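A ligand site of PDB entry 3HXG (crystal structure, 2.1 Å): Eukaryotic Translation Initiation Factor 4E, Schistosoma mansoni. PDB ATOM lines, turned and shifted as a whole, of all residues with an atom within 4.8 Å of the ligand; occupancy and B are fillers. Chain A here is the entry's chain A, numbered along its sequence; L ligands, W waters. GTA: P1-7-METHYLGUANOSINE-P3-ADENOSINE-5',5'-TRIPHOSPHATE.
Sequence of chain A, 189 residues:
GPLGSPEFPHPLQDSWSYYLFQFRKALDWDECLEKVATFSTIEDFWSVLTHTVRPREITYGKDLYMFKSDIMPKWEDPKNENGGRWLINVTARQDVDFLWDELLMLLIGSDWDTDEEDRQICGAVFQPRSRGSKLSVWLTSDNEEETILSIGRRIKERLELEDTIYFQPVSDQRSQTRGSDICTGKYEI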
ATOM      1  N   PHE A  21      -9.984  -8.811 -20.444  1.00  0.00           N
ATOM      2  CA  PHE A  21     -10.626  -9.536 -21.523  1.00  0.00           C
ATOM      3  C   PHE A  21     -11.971 -10.044 -21.005  1.00  0.00           C
ATOM      4  O   PHE A  21     -12.026 -10.702 -19.974  1.00  0.00           O
ATOM      5  CB  PHE A  21      -9.729 -10.689 -22.014  1.00  0.00           C
ATOM      6  CG  PHE A  21     -10.392 -11.583 -23.036  1.00  0.00           C
ATOM      7  CD1 PHE A  21     -10.234 -11.338 -24.398  1.00  0.00           C
ATOM      8  CD2 PHE A  21     -11.169 -12.666 -22.621  1.00  0.00           C
ATOM      9  CE1 PHE A  21     -10.850 -12.154 -25.335  1.00  0.00           C
ATOM     10  CE2 PHE A  21     -11.783 -13.496 -23.562  1.00  0.00           C
ATOM     11  CZ  PHE A  21     -11.627 -13.237 -24.920  1.00  0.00           C
ATOM     12  N   PHE A  23     -15.404 -11.892 -22.733  1.00  0.00           N
ATOM     13  CA  PHE A  23     -16.102 -12.371 -23.913  1.00  0.00           C
ATOM     14  C   PHE A  23     -17.588 -12.002 -23.900  1.00  0.00           C
ATOM     15  O   PHE A  23     -18.269 -12.176 -22.883  1.00  0.00           O
ATOM     16  CB  PHE A  23     -15.940 -13.887 -24.105  1.00  0.00           C
ATOM     17  CG  PHE A  23     -16.822 -14.449 -25.192  1.00  0.00           C
ATOM     18  CD1 PHE A  23     -16.454 -14.309 -26.533  1.00  0.00           C
ATOM     19  CD2 PHE A  23     -18.017 -15.081 -24.888  1.00  0.00           C
ATOM     20  CE1 PHE A  23     -17.260 -14.820 -27.548  1.00  0.00           C
ATOM     21  CE2 PHE A  23     -18.828 -15.600 -25.886  1.00  0.00           C
ATOM     22  CZ  PHE A  23     -18.448 -15.460 -27.222  1.00  0.00           C
ATOM     23  N   LEU A  27     -18.629 -10.494 -30.622  1.00  0.00           N
ATOM     24  CA  LEU A  27     -17.363  -9.763 -30.651  1.00  0.00           C
ATOM     25  C   LEU A  27     -16.235 -10.719 -31.020  1.00  0.00           C
ATOM     26  O   LEU A  27     -16.204 -11.881 -30.583  1.00  0.00           O
ATOM     27  CB  LEU A  27     -17.050  -9.118 -29.302  1.00  0.00           C
ATOM     28  CG  LEU A  27     -17.983  -8.024 -28.769  1.00  0.00           C
ATOM     29  CD1 LEU A  27     -17.670  -7.792 -27.308  1.00  0.00           C
ATOM     30  CD2 LEU A  27     -17.866  -6.724 -29.563  1.00  0.00           C
ATOM     31  N   ASP A  28     -15.312 -10.221 -31.858  1.00  0.00           N
ATOM     32  CA  ASP A  28     -14.097 -10.955 -32.204  1.00  0.00           C
ATOM     33  C   ASP A  28     -13.189 -10.980 -30.977  1.00  0.00           C
ATOM     34  O   ASP A  28     -13.346 -10.185 -30.057  1.00  0.00           O
ATOM     35  CB  ASP A  28     -13.370 -10.298 -33.379  1.00  0.00           C
ATOM     36  CG  ASP A  28     -14.178 -10.327 -34.684  1.00  0.00           C
ATOM     37  OD1 ASP A  28     -15.080 -11.168 -34.819  1.00  0.00           O
ATOM     38  OD2 ASP A  28     -13.901  -9.499 -35.562  1.00  0.00           O
ATOM     39  N   TRP A  29     -12.237 -11.919 -30.968  1.00  0.00           N
ATOM     40  CA  TRP A  29     -11.332 -12.062 -29.837  1.00  0.00           C
ATOM     41  C   TRP A  29     -10.757 -10.707 -29.409  1.00  0.00           C
ATOM     42  O   TRP A  29     -10.878 -10.322 -28.238  1.00  0.00           O
ATOM     43  CB  TRP A  29     -10.217 -13.080 -30.123  1.00  0.00           C
ATOM     44  CG  TRP A  29      -9.390 -13.333 -28.873  1.00  0.00           C
ATOM     45  CD1 TRP A  29      -9.651 -14.249 -27.889  1.00  0.00           C
ATOM     46  CD2 TRP A  29      -8.213 -12.619 -28.472  1.00  0.00           C
ATOM     47  NE1 TRP A  29      -8.697 -14.159 -26.894  1.00  0.00           N
ATOM     48  CE2 TRP A  29      -7.801 -13.165 -27.234  1.00  0.00           C
ATOM     49  CE3 TRP A  29      -7.458 -11.584 -29.042  1.00  0.00           C
ATOM     50  CZ2 TRP A  29      -6.677 -12.699 -26.546  1.00  0.00           C
ATOM     51  CZ3 TRP A  29      -6.331 -11.115 -28.362  1.00  0.00           C
ATOM     52  CH2 TRP A  29      -5.957 -11.677 -27.122  1.00  0.00           C
ATOM     53  N   GLY A  61     -12.958 -17.219 -17.156  1.00  0.00           N
ATOM     54  CA  GLY A  61     -12.910 -16.808 -18.569  1.00  0.00           C
ATOM     55  C   GLY A  61     -12.745 -15.315 -18.806  1.00  0.00           C
ATOM     56  O   GLY A  61     -12.704 -14.873 -19.968  1.00  0.00           O
ATOM     57  N   ASP A  63     -10.163 -12.366 -18.287  1.00  0.00           N
ATOM     58  CA  ASP A  63      -8.705 -12.429 -18.146  1.00  0.00           C
ATOM     59  C   ASP A  63      -8.061 -11.058 -17.939  1.00  0.00           C
ATOM     60  O   ASP A  63      -8.627 -10.034 -18.309  1.00  0.00           O
ATOM     61  CB  ASP A  63      -8.086 -13.122 -19.370  1.00  0.00           C
ATOM     62  CG  ASP A  63      -8.547 -14.566 -19.530  1.00  0.00           C
ATOM     63  OD1 ASP A  63      -9.242 -15.066 -18.632  1.00  0.00           O
ATOM     64  OD2 ASP A  63      -8.220 -15.185 -20.577  1.00  0.00           O
ATOM     65  N   TYR A  65      -4.562  -8.829 -18.626  1.00  0.00           N
ATOM     66  CA  TYR A  65      -3.353  -8.660 -19.441  1.00  0.00           C
ATOM     67  C   TYR A  65      -2.634  -7.380 -19.003  1.00  0.00           C
ATOM     68  O   TYR A  65      -3.245  -6.302 -18.967  1.00  0.00           O
ATOM     69  CB  TYR A  65      -3.713  -8.536 -20.941  1.00  0.00           C
ATOM     70  CG  TYR A  65      -4.183  -9.818 -21.609  1.00  0.00           C
ATOM     71  CD1 TYR A  65      -3.338 -10.505 -22.494  1.00  0.00           C
ATOM     72  CD2 TYR A  65      -5.463 -10.350 -21.374  1.00  0.00           C
ATOM     73  CE1 TYR A  65      -3.741 -11.670 -23.134  1.00  0.00           C
ATOM     74  CE2 TYR A  65      -5.885 -11.539 -22.020  1.00  0.00           C
ATOM     75  CZ  TYR A  65      -5.010 -12.189 -22.890  1.00  0.00           C
ATOM     76  OH  TYR A  65      -5.371 -13.365 -23.519  1.00  0.00           O
ATOM     77  N   PRO A  73      -1.715  -6.329 -26.403  1.00  0.00           N
ATOM     78  CA  PRO A  73      -1.776  -7.663 -25.786  1.00  0.00           C
ATOM     79  C   PRO A  73      -2.364  -8.732 -26.728  1.00  0.00           C
ATOM     80  O   PRO A  73      -3.404  -9.333 -26.434  1.00  0.00           O
ATOM     81  CB  PRO A  73      -2.664  -7.432 -24.558  1.00  0.00           C
ATOM     82  CG  PRO A  73      -3.573  -6.326 -24.951  1.00  0.00           C
ATOM     83  CD  PRO A  73      -2.837  -5.474 -25.960  1.00  0.00           C
ATOM     84  N   LYS A  74      -1.685  -8.980 -27.844  1.00  0.00           N
ATOM     85  CA  LYS A  74      -2.150  -9.914 -28.844  1.00  0.00           C
ATOM     86  C   LYS A  74      -0.963 -10.475 -29.609  1.00  0.00           C
ATOM     87  O   LYS A  74       0.065  -9.805 -29.740  1.00  0.00           O
ATOM     88  CB  LYS A  74      -3.154  -9.233 -29.806  1.00  0.00           C
ATOM     89  CG  LYS A  74      -2.543  -8.166 -30.713  1.00  0.00           C
ATOM     90  CD  LYS A  74      -3.566  -7.539 -31.659  1.00  0.00           C
ATOM     91  CE  LYS A  74      -2.872  -6.613 -32.664  1.00  0.00           C
ATOM     92  NZ  LYS A  74      -3.670  -6.292 -33.920  1.00  0.00           N
ATOM     93  N   TRP A  75      -1.092 -11.708 -30.108  1.00  0.00           N
ATOM     94  CA  TRP A  75      -0.023 -12.352 -30.870  1.00  0.00           C
ATOM     95  C   TRP A  75       0.397 -11.534 -32.078  1.00  0.00           C
ATOM     96  O   TRP A  75       1.536 -11.616 -32.521  1.00  0.00           O
ATOM     97  CB  TRP A  75      -0.476 -13.719 -31.396  1.00  0.00           C
ATOM     98  CG  TRP A  75      -0.807 -14.752 -30.373  1.00  0.00           C
ATOM     99  CD1 TRP A  75      -0.171 -15.004 -29.181  1.00  0.00           C
ATOM    100  CD2 TRP A  75      -1.841 -15.742 -30.482  1.00  0.00           C
ATOM    101  NE1 TRP A  75      -0.775 -16.055 -28.528  1.00  0.00           N
ATOM    102  CE2 TRP A  75      -1.801 -16.530 -29.311  1.00  0.00           C
ATOM    103  CE3 TRP A  75      -2.816 -16.016 -31.459  1.00  0.00           C
ATOM    104  CZ2 TRP A  75      -2.689 -17.582 -29.084  1.00  0.00           C
ATOM    105  CZ3 TRP A  75      -3.699 -17.061 -31.227  1.00  0.00           C
ATOM    106  CH2 TRP A  75      -3.631 -17.832 -30.050  1.00  0.00           C
ATOM    107  N   GLU A  76      -0.542 -10.757 -32.609  1.00  0.00           N
ATOM    108  CA  GLU A  76      -0.316 -10.038 -33.873  1.00  0.00           C
ATOM    109  C   GLU A  76       0.673  -8.864 -33.748  1.00  0.00           C
ATOM    110  O   GLU A  76       1.276  -8.451 -34.750  1.00  0.00           O
ATOM    111  CB  GLU A  76      -1.660  -9.593 -34.475  1.00  0.00           C
ATOM    112  CG  GLU A  76      -2.545 -10.746 -34.988  1.00  0.00           C
ATOM    113  CD  GLU A  76      -3.148 -11.636 -33.889  1.00  0.00           C
ATOM    114  OE1 GLU A  76      -3.388 -11.177 -32.753  1.00  0.00           O
ATOM    115  OE2 GLU A  76      -3.397 -12.836 -34.178  1.00  0.00           O
ATOM    116  N   ARG A  85       5.561 -17.644 -24.622  1.00  0.00           N
ATOM    117  CA  ARG A  85       5.186 -17.408 -23.228  1.00  0.00           C
ATOM    118  C   ARG A  85       5.730 -18.488 -22.305  1.00  0.00           C
ATOM    119  O   ARG A  85       5.836 -19.650 -22.711  1.00  0.00           O
ATOM    120  CB  ARG A  85       3.654 -17.315 -23.085  1.00  0.00           C
ATOM    121  CG  ARG A  85       2.965 -18.661 -23.276  1.00  0.00           C
ATOM    122  CD  ARG A  85       1.461 -18.566 -23.145  1.00  0.00           C
ATOM    123  NE  ARG A  85       0.859 -19.884 -23.372  1.00  0.00           N
ATOM    124  CZ  ARG A  85      -0.427 -20.169 -23.150  1.00  0.00           C
ATOM    125  NH1 ARG A  85      -0.875 -21.391 -23.372  1.00  0.00           N
ATOM    126  NH2 ARG A  85      -1.260 -19.225 -22.701  1.00  0.00           N
ATOM    127  N   GLN A 127      -5.338 -15.971 -16.371  1.00  0.00           N
ATOM    128  CA  GLN A 127      -6.514 -16.612 -16.980  1.00  0.00           C
ATOM    129  C   GLN A 127      -7.174 -17.592 -15.997  1.00  0.00           C
ATOM    130  O   GLN A 127      -6.691 -18.711 -15.812  1.00  0.00           O
ATOM    131  CB  GLN A 127      -6.110 -17.335 -18.272  1.00  0.00           C
ATOM    132  CG  GLN A 127      -5.555 -16.409 -19.350  1.00  0.00           C
ATOM    133  CD  GLN A 127      -5.069 -17.156 -20.576  1.00  0.00           C
ATOM    134  OE1 GLN A 127      -4.148 -17.972 -20.503  1.00  0.00           O
ATOM    135  NE2 GLN A 127      -5.693 -16.870 -21.726  1.00  0.00           N
ATOM    136  N   ARG A 129      -9.666 -20.309 -14.850  1.00  0.00           N
ATOM    137  CA  ARG A 129     -10.374 -21.377 -15.537  1.00  0.00           C
ATOM    138  C   ARG A 129     -10.830 -22.423 -14.542  1.00  0.00           C
ATOM    139  O   ARG A 129     -10.080 -22.800 -13.648  1.00  0.00           O
ATOM    140  CB  ARG A 129      -9.471 -22.061 -16.573  1.00  0.00           C
ATOM    141  CG  ARG A 129      -8.915 -21.181 -17.670  1.00  0.00           C
ATOM    142  CD  ARG A 129     -10.001 -20.714 -18.627  1.00  0.00           C
ATOM    143  NE  ARG A 129      -9.419 -19.929 -19.720  1.00  0.00           N
ATOM    144  CZ  ARG A 129      -9.250 -18.615 -19.710  1.00  0.00           C
ATOM    145  NH1 ARG A 129      -8.692 -18.019 -20.755  1.00  0.00           N
ATOM    146  NH2 ARG A 129      -9.612 -17.894 -18.645  1.00  0.00           N
ATOM    147  N   LYS A 134      -4.389 -20.251 -15.298  1.00  0.00           N
ATOM    148  CA  LYS A 134      -3.076 -20.106 -15.925  1.00  0.00           C
ATOM    149  C   LYS A 134      -2.522 -18.704 -15.726  1.00  0.00           C
ATOM    150  O   LYS A 134      -3.258 -17.722 -15.787  1.00  0.00           O
ATOM    151  CB  LYS A 134      -3.169 -20.402 -17.436  1.00  0.00           C
ATOM    152  CG  LYS A 134      -3.560 -21.846 -17.799  1.00  0.00           C
ATOM    153  CD  LYS A 134      -3.866 -22.007 -19.286  1.00  0.00           C
ATOM    154  CE  LYS A 134      -5.295 -21.561 -19.609  1.00  0.00           C
ATOM    155  NZ  LYS A 134      -5.629 -21.852 -21.046  1.00  0.00           N
ATOM    156  N   TRP A 138       4.726 -13.282 -21.424  1.00  0.00           N
ATOM    157  CA  TRP A 138       4.994 -13.252 -22.849  1.00  0.00           C
ATOM    158  C   TRP A 138       6.324 -12.577 -23.073  1.00  0.00           C
ATOM    159  O   TRP A 138       6.611 -11.511 -22.495  1.00  0.00           O
ATOM    160  CB  TRP A 138       3.923 -12.439 -23.573  1.00  0.00           C
ATOM    161  CG  TRP A 138       2.602 -13.133 -23.720  1.00  0.00           C
ATOM    162  CD1 TRP A 138       2.028 -14.043 -22.871  1.00  0.00           C
ATOM    163  CD2 TRP A 138       1.658 -12.924 -24.780  1.00  0.00           C
ATOM    164  NE1 TRP A 138       0.791 -14.419 -23.334  1.00  0.00           N
ATOM    165  CE2 TRP A 138       0.549 -13.754 -24.517  1.00  0.00           C
ATOM    166  CE3 TRP A 138       1.644 -12.117 -25.922  1.00  0.00           C
ATOM    167  CZ2 TRP A 138      -0.572 -13.806 -25.362  1.00  0.00           C
ATOM    168  CZ3 TRP A 138       0.528 -12.162 -26.762  1.00  0.00           C
ATOM    169  CH2 TRP A 138      -0.550 -13.001 -26.480  1.00  0.00           C
ATOM    170  N   GLN A 176      -2.729 -24.509 -30.959  1.00  0.00           N
ATOM    171  CA  GLN A 176      -3.304 -25.234 -29.814  1.00  0.00           C
ATOM    172  C   GLN A 176      -4.834 -25.241 -29.839  1.00  0.00           C
ATOM    173  O   GLN A 176      -5.484 -24.196 -29.796  1.00  0.00           O
ATOM    174  CB  GLN A 176      -2.803 -24.629 -28.493  1.00  0.00           C
ATOM    175  CG  GLN A 176      -3.499 -25.149 -27.238  1.00  0.00           C
ATOM    176  CD  GLN A 176      -2.996 -26.506 -26.802  1.00  0.00           C
ATOM    177  OE1 GLN A 176      -1.937 -26.960 -27.247  1.00  0.00           O
ATOM    178  NE2 GLN A 176      -3.742 -27.165 -25.910  1.00  0.00           N
ATOM    179  N   ARG A 178      -8.425 -25.627 -28.430  1.00  0.00           N
ATOM    180  CA  ARG A 178      -9.137 -25.447 -27.160  1.00  0.00           C
ATOM    181  C   ARG A 178      -9.637 -26.806 -26.680  1.00  0.00           C
ATOM    182  O   ARG A 178     -10.147 -27.613 -27.482  1.00  0.00           O
ATOM    183  CB  ARG A 178     -10.303 -24.476 -27.326  1.00  0.00           C
ATOM    184  CG  ARG A 178      -9.905 -23.014 -27.571  1.00  0.00           C
ATOM    185  CD  ARG A 178     -11.060 -22.220 -28.174  1.00  0.00           C
ATOM    186  NE  ARG A 178     -12.202 -22.078 -27.260  1.00  0.00           N
ATOM    187  CZ  ARG A 178     -13.463 -21.872 -27.635  1.00  0.00           C
ATOM    188  NH1 ARG A 178     -13.775 -21.794 -28.920  1.00  0.00           N
ATOM    189  NH2 ARG A 178     -14.429 -21.766 -26.719  1.00  0.00           N
ATOM    190  N   GLY A 179      -9.463 -27.073 -25.388  1.00  0.00           N
ATOM    191  CA  GLY A 179      -9.964 -28.317 -24.803  1.00  0.00           C
ATOM    192  C   GLY A 179      -8.949 -29.429 -24.683  1.00  0.00           C
ATOM    193  O   GLY A 179      -9.143 -30.363 -23.889  1.00  0.00           O
HETATM  194  N2  GTA L   1      -6.103 -13.467 -32.927  1.00  0.00           N
HETATM  195  O6  GTA L   1      -3.408 -13.033 -29.271  1.00  0.00           O
HETATM  196  C6  GTA L   1      -4.403 -13.589 -29.789  1.00  0.00           C
HETATM  197  C5  GTA L   1      -5.184 -14.556 -29.143  1.00  0.00           C
HETATM  198  N7  GTA L   1      -5.089 -15.083 -27.910  1.00  0.00           N
HETATM  199  C7  GTA L   1      -4.084 -14.784 -26.855  1.00  0.00           C
HETATM  200  C8  GTA L   1      -6.084 -15.984 -27.796  1.00  0.00           C
HETATM  201  N9  GTA L   1      -6.794 -16.014 -28.940  1.00  0.00           N
HETATM  202  C4  GTA L   1      -6.260 -15.137 -29.783  1.00  0.00           C
HETATM  203  N3  GTA L   1      -6.546 -14.770 -31.050  1.00  0.00           N
HETATM  204  C2  GTA L   1      -5.801 -13.829 -31.663  1.00  0.00           C
HETATM  205  N1  GTA L   1      -4.751 -13.266 -31.052  1.00  0.00           N
HETATM  206  O3A GTA L   1      -7.629 -20.474 -29.296  1.00  0.00           O
HETATM  207  C1A GTA L   1      -7.978 -16.861 -29.250  1.00  0.00           C
HETATM  208  C2A GTA L   1      -7.517 -18.134 -29.951  1.00  0.00           C
HETATM  209  C3A GTA L   1      -7.485 -19.143 -28.830  1.00  0.00           C
HETATM  210  C4A GTA L   1      -8.679 -18.700 -28.015  1.00  0.00           C
HETATM  211  C5A GTA L   1      -8.601 -19.178 -26.585  1.00  0.00           C
HETATM  212  O4A GTA L   1      -8.627 -17.278 -28.048  1.00  0.00           O
HETATM  213  O2A GTA L   1      -8.475 -18.517 -30.979  1.00  0.00           O
HETATM  214  P1  GTA L   1      -7.119 -18.951 -24.479  1.00  0.00           P
HETATM  215  O11 GTA L   1      -5.669 -18.606 -24.227  1.00  0.00           O
HETATM  216  O12 GTA L   1      -8.217 -18.187 -23.791  1.00  0.00           O
HETATM  217  O13 GTA L   1      -7.262 -20.532 -24.306  1.00  0.00           O
HETATM  218  O15 GTA L   1      -7.345 -18.793 -26.053  1.00  0.00           O
HETATM  219  P2  GTA L   1      -8.309 -21.325 -23.386  1.00  0.00           P
HETATM  220  O22 GTA L   1      -8.201 -22.774 -23.821  1.00  0.00           O
HETATM  221  O21 GTA L   1      -8.064 -20.923 -21.946  1.00  0.00           O
HETATM  222  O23 GTA L   1      -9.730 -20.798 -23.936  1.00  0.00           O
HETATM  223  P3  GTA L   1     -11.178 -21.210 -23.357  1.00  0.00           P
HETATM  224  O32 GTA L   1     -11.822 -22.096 -24.391  1.00  0.00           O
HETATM  225  O31 GTA L   1     -11.160 -21.665 -21.915  1.00  0.00           O
HETATM  226  O33 GTA L   1     -11.917 -19.781 -23.368  1.00  0.00           O
HETATM  227  C5B GTA L   1     -11.541 -18.706 -22.489  1.00  0.00           C
HETATM  228  C4B GTA L   1     -12.378 -17.458 -22.773  1.00  0.00           C
HETATM  229  O4B GTA L   1     -12.078 -16.968 -24.083  1.00  0.00           O
HETATM  230  C3B GTA L   1     -13.872 -17.690 -22.765  1.00  0.00           C
HETATM  231  O3B GTA L   1     -14.487 -16.474 -22.305  1.00  0.00           O
HETATM  232  C2B GTA L   1     -14.255 -17.930 -24.221  1.00  0.00           C
HETATM  233  O2B GTA L   1     -15.598 -17.520 -24.506  1.00  0.00           O
HETATM  234  C1B GTA L   1     -13.236 -17.035 -24.925  1.00  0.00           C
HETATM  235  N9C GTA L   1     -12.787 -17.512 -26.245  1.00  0.00           N
HETATM  236  C8C GTA L   1     -12.220 -18.700 -26.528  1.00  0.00           C
HETATM  237  N7C GTA L   1     -11.894 -18.787 -27.831  1.00  0.00           N
HETATM  238  C5C GTA L   1     -12.226 -17.606 -28.393  1.00  0.00           C
HETATM  239  C6C GTA L   1     -12.154 -17.018 -29.734  1.00  0.00           C
HETATM  240  N6C GTA L   1     -11.637 -17.720 -30.769  1.00  0.00           N
HETATM  241  N1C GTA L   1     -12.637 -15.756 -29.894  1.00  0.00           N
HETATM  242  C2C GTA L   1     -13.163 -15.033 -28.876  1.00  0.00           C
HETATM  243  N3C GTA L   1     -13.260 -15.511 -27.624  1.00  0.00           N
HETATM  244  C4C GTA L   1     -12.817 -16.771 -27.341  1.00  0.00           C
HETATM  245  O   HOH W   1      -9.300 -15.904 -24.587  1.00  0.00           O
HETATM  246  O   HOH W   2      -3.858 -19.096 -26.027  1.00  0.00           O
HETATM  247  O   HOH W   3      -6.459 -23.368 -25.725  1.00  0.00           O
HETATM  248  O   HOH W   4     -14.864 -13.692 -20.707  1.00  0.00           O
HETATM  249  O   HOH W   5     -13.010 -14.435 -32.371  1.00  0.00           O
HETATM  250  O   HOH W   6     -10.249 -23.771 -20.421  1.00  0.00           O
HETATM  251  O   HOH W   7      -9.015 -25.300 -23.605  1.00  0.00           O
HETATM  252  O   HOH W   8     -12.981 -20.478 -19.939  1.00  0.00           O
HETATM  253  O   HOH W   9      -8.183 -16.616 -32.796  1.00  0.00           O
HETATM  254  O   HOH W  10      -6.253 -22.300 -28.177  1.00  0.00           O
HETATM  255  O   HOH W  11      -4.092 -19.789 -22.350  1.00  0.00           O
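NZ of Lys 134 is in salt-bridge range of O21 of the ligand (2.8 Å). The guanidinium group (NE) of Arg 129 lies within salt-bridge range of an oxygen (O21) of the ligand (2.8 Å). The backbone NH of Trp 75 lies within hydrogen-bond range of an oxygen (O6) of the ligand (2.8 Å). O32 of the ligand is in salt-bridge range of NE of Arg 178. The side-chain carboxylate (OE1) of Glu 76 is in hydrogen-bond range of a nitrogen (N1) of the ligand (3.0 Å). O11 of the ligand is in hydrogen-bond range of NE2 of Gln 127, at 3.0 Å. O4A of the ligand sits close to NE1 of Trp 29. The backbone carbonyl oxygen of Gly 61 is in hydrogen-bond range of an oxygen (O3B) of the ligand (3.3 Å).
O of Lys 134 sits at hydrogen-bond distance from N of Gln 127 (2.8 Å). NE2 of Gln 127 lies close to NH1 of Arg 129. OD1 of Asp 63 lies within salt-bridge range of NH2 of Arg 129 (2.9 Å). The side-chain carboxylate of Asp 63 lies close to the side-chain amide nitrogen of Gln 127 (3.2 Å). The backbone carbonyl oxygen of Asp 63 lies within hydrogen-bond range of the backbone NH of Phe 21 (2.8 Å).
Residues that only touch the ligand: Phe 23 (3.4 Å), Lys 74 (3.4 Å), Phe 21 (3.5 Å), Tyr 65 (3.8 Å) and Trp 138 (3.9 Å). Hydrophobic or aromatic side chains that line the ligand: Phe 21, Phe 23, Trp 29, Trp 75 and Trp 138. Of the 20 residues printed, 13 come within 4 Å of the ligand.
Water W10 bridges O3A of the ligand (2.5 Å) and O of Gln 176 (2.6 Å). Water W1 lies within hydrogen-bond range of an oxygen (O12) of the ligand (2.6 Å) and the indole nitrogen (NE1) of Trp 29 (3.0 Å). Water W7 lies within hydrogen-bond range of N of Gly 179 and O22 of the ligand. Water W11 lies within hydrogen-bond range of the side-chain amide oxygen of Gln 127 (2.6 Å), an oxygen (O11) of the ligand (2.7 Å), the side-chain amino group of Lys 134 (2.9 Å) and the guanidinium group of Arg 85 (2.9 Å). Water W5 lies within hydrogen-bond range of N1C of the ligand (2.8 Å) and N of Trp 29 (3.0 Å). Water W4 lies within hydrogen-bond range of O of Gly 61 (2.6 Å), N of Phe 23 (2.8 Å) and O3B of the ligand (3.2 Å).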
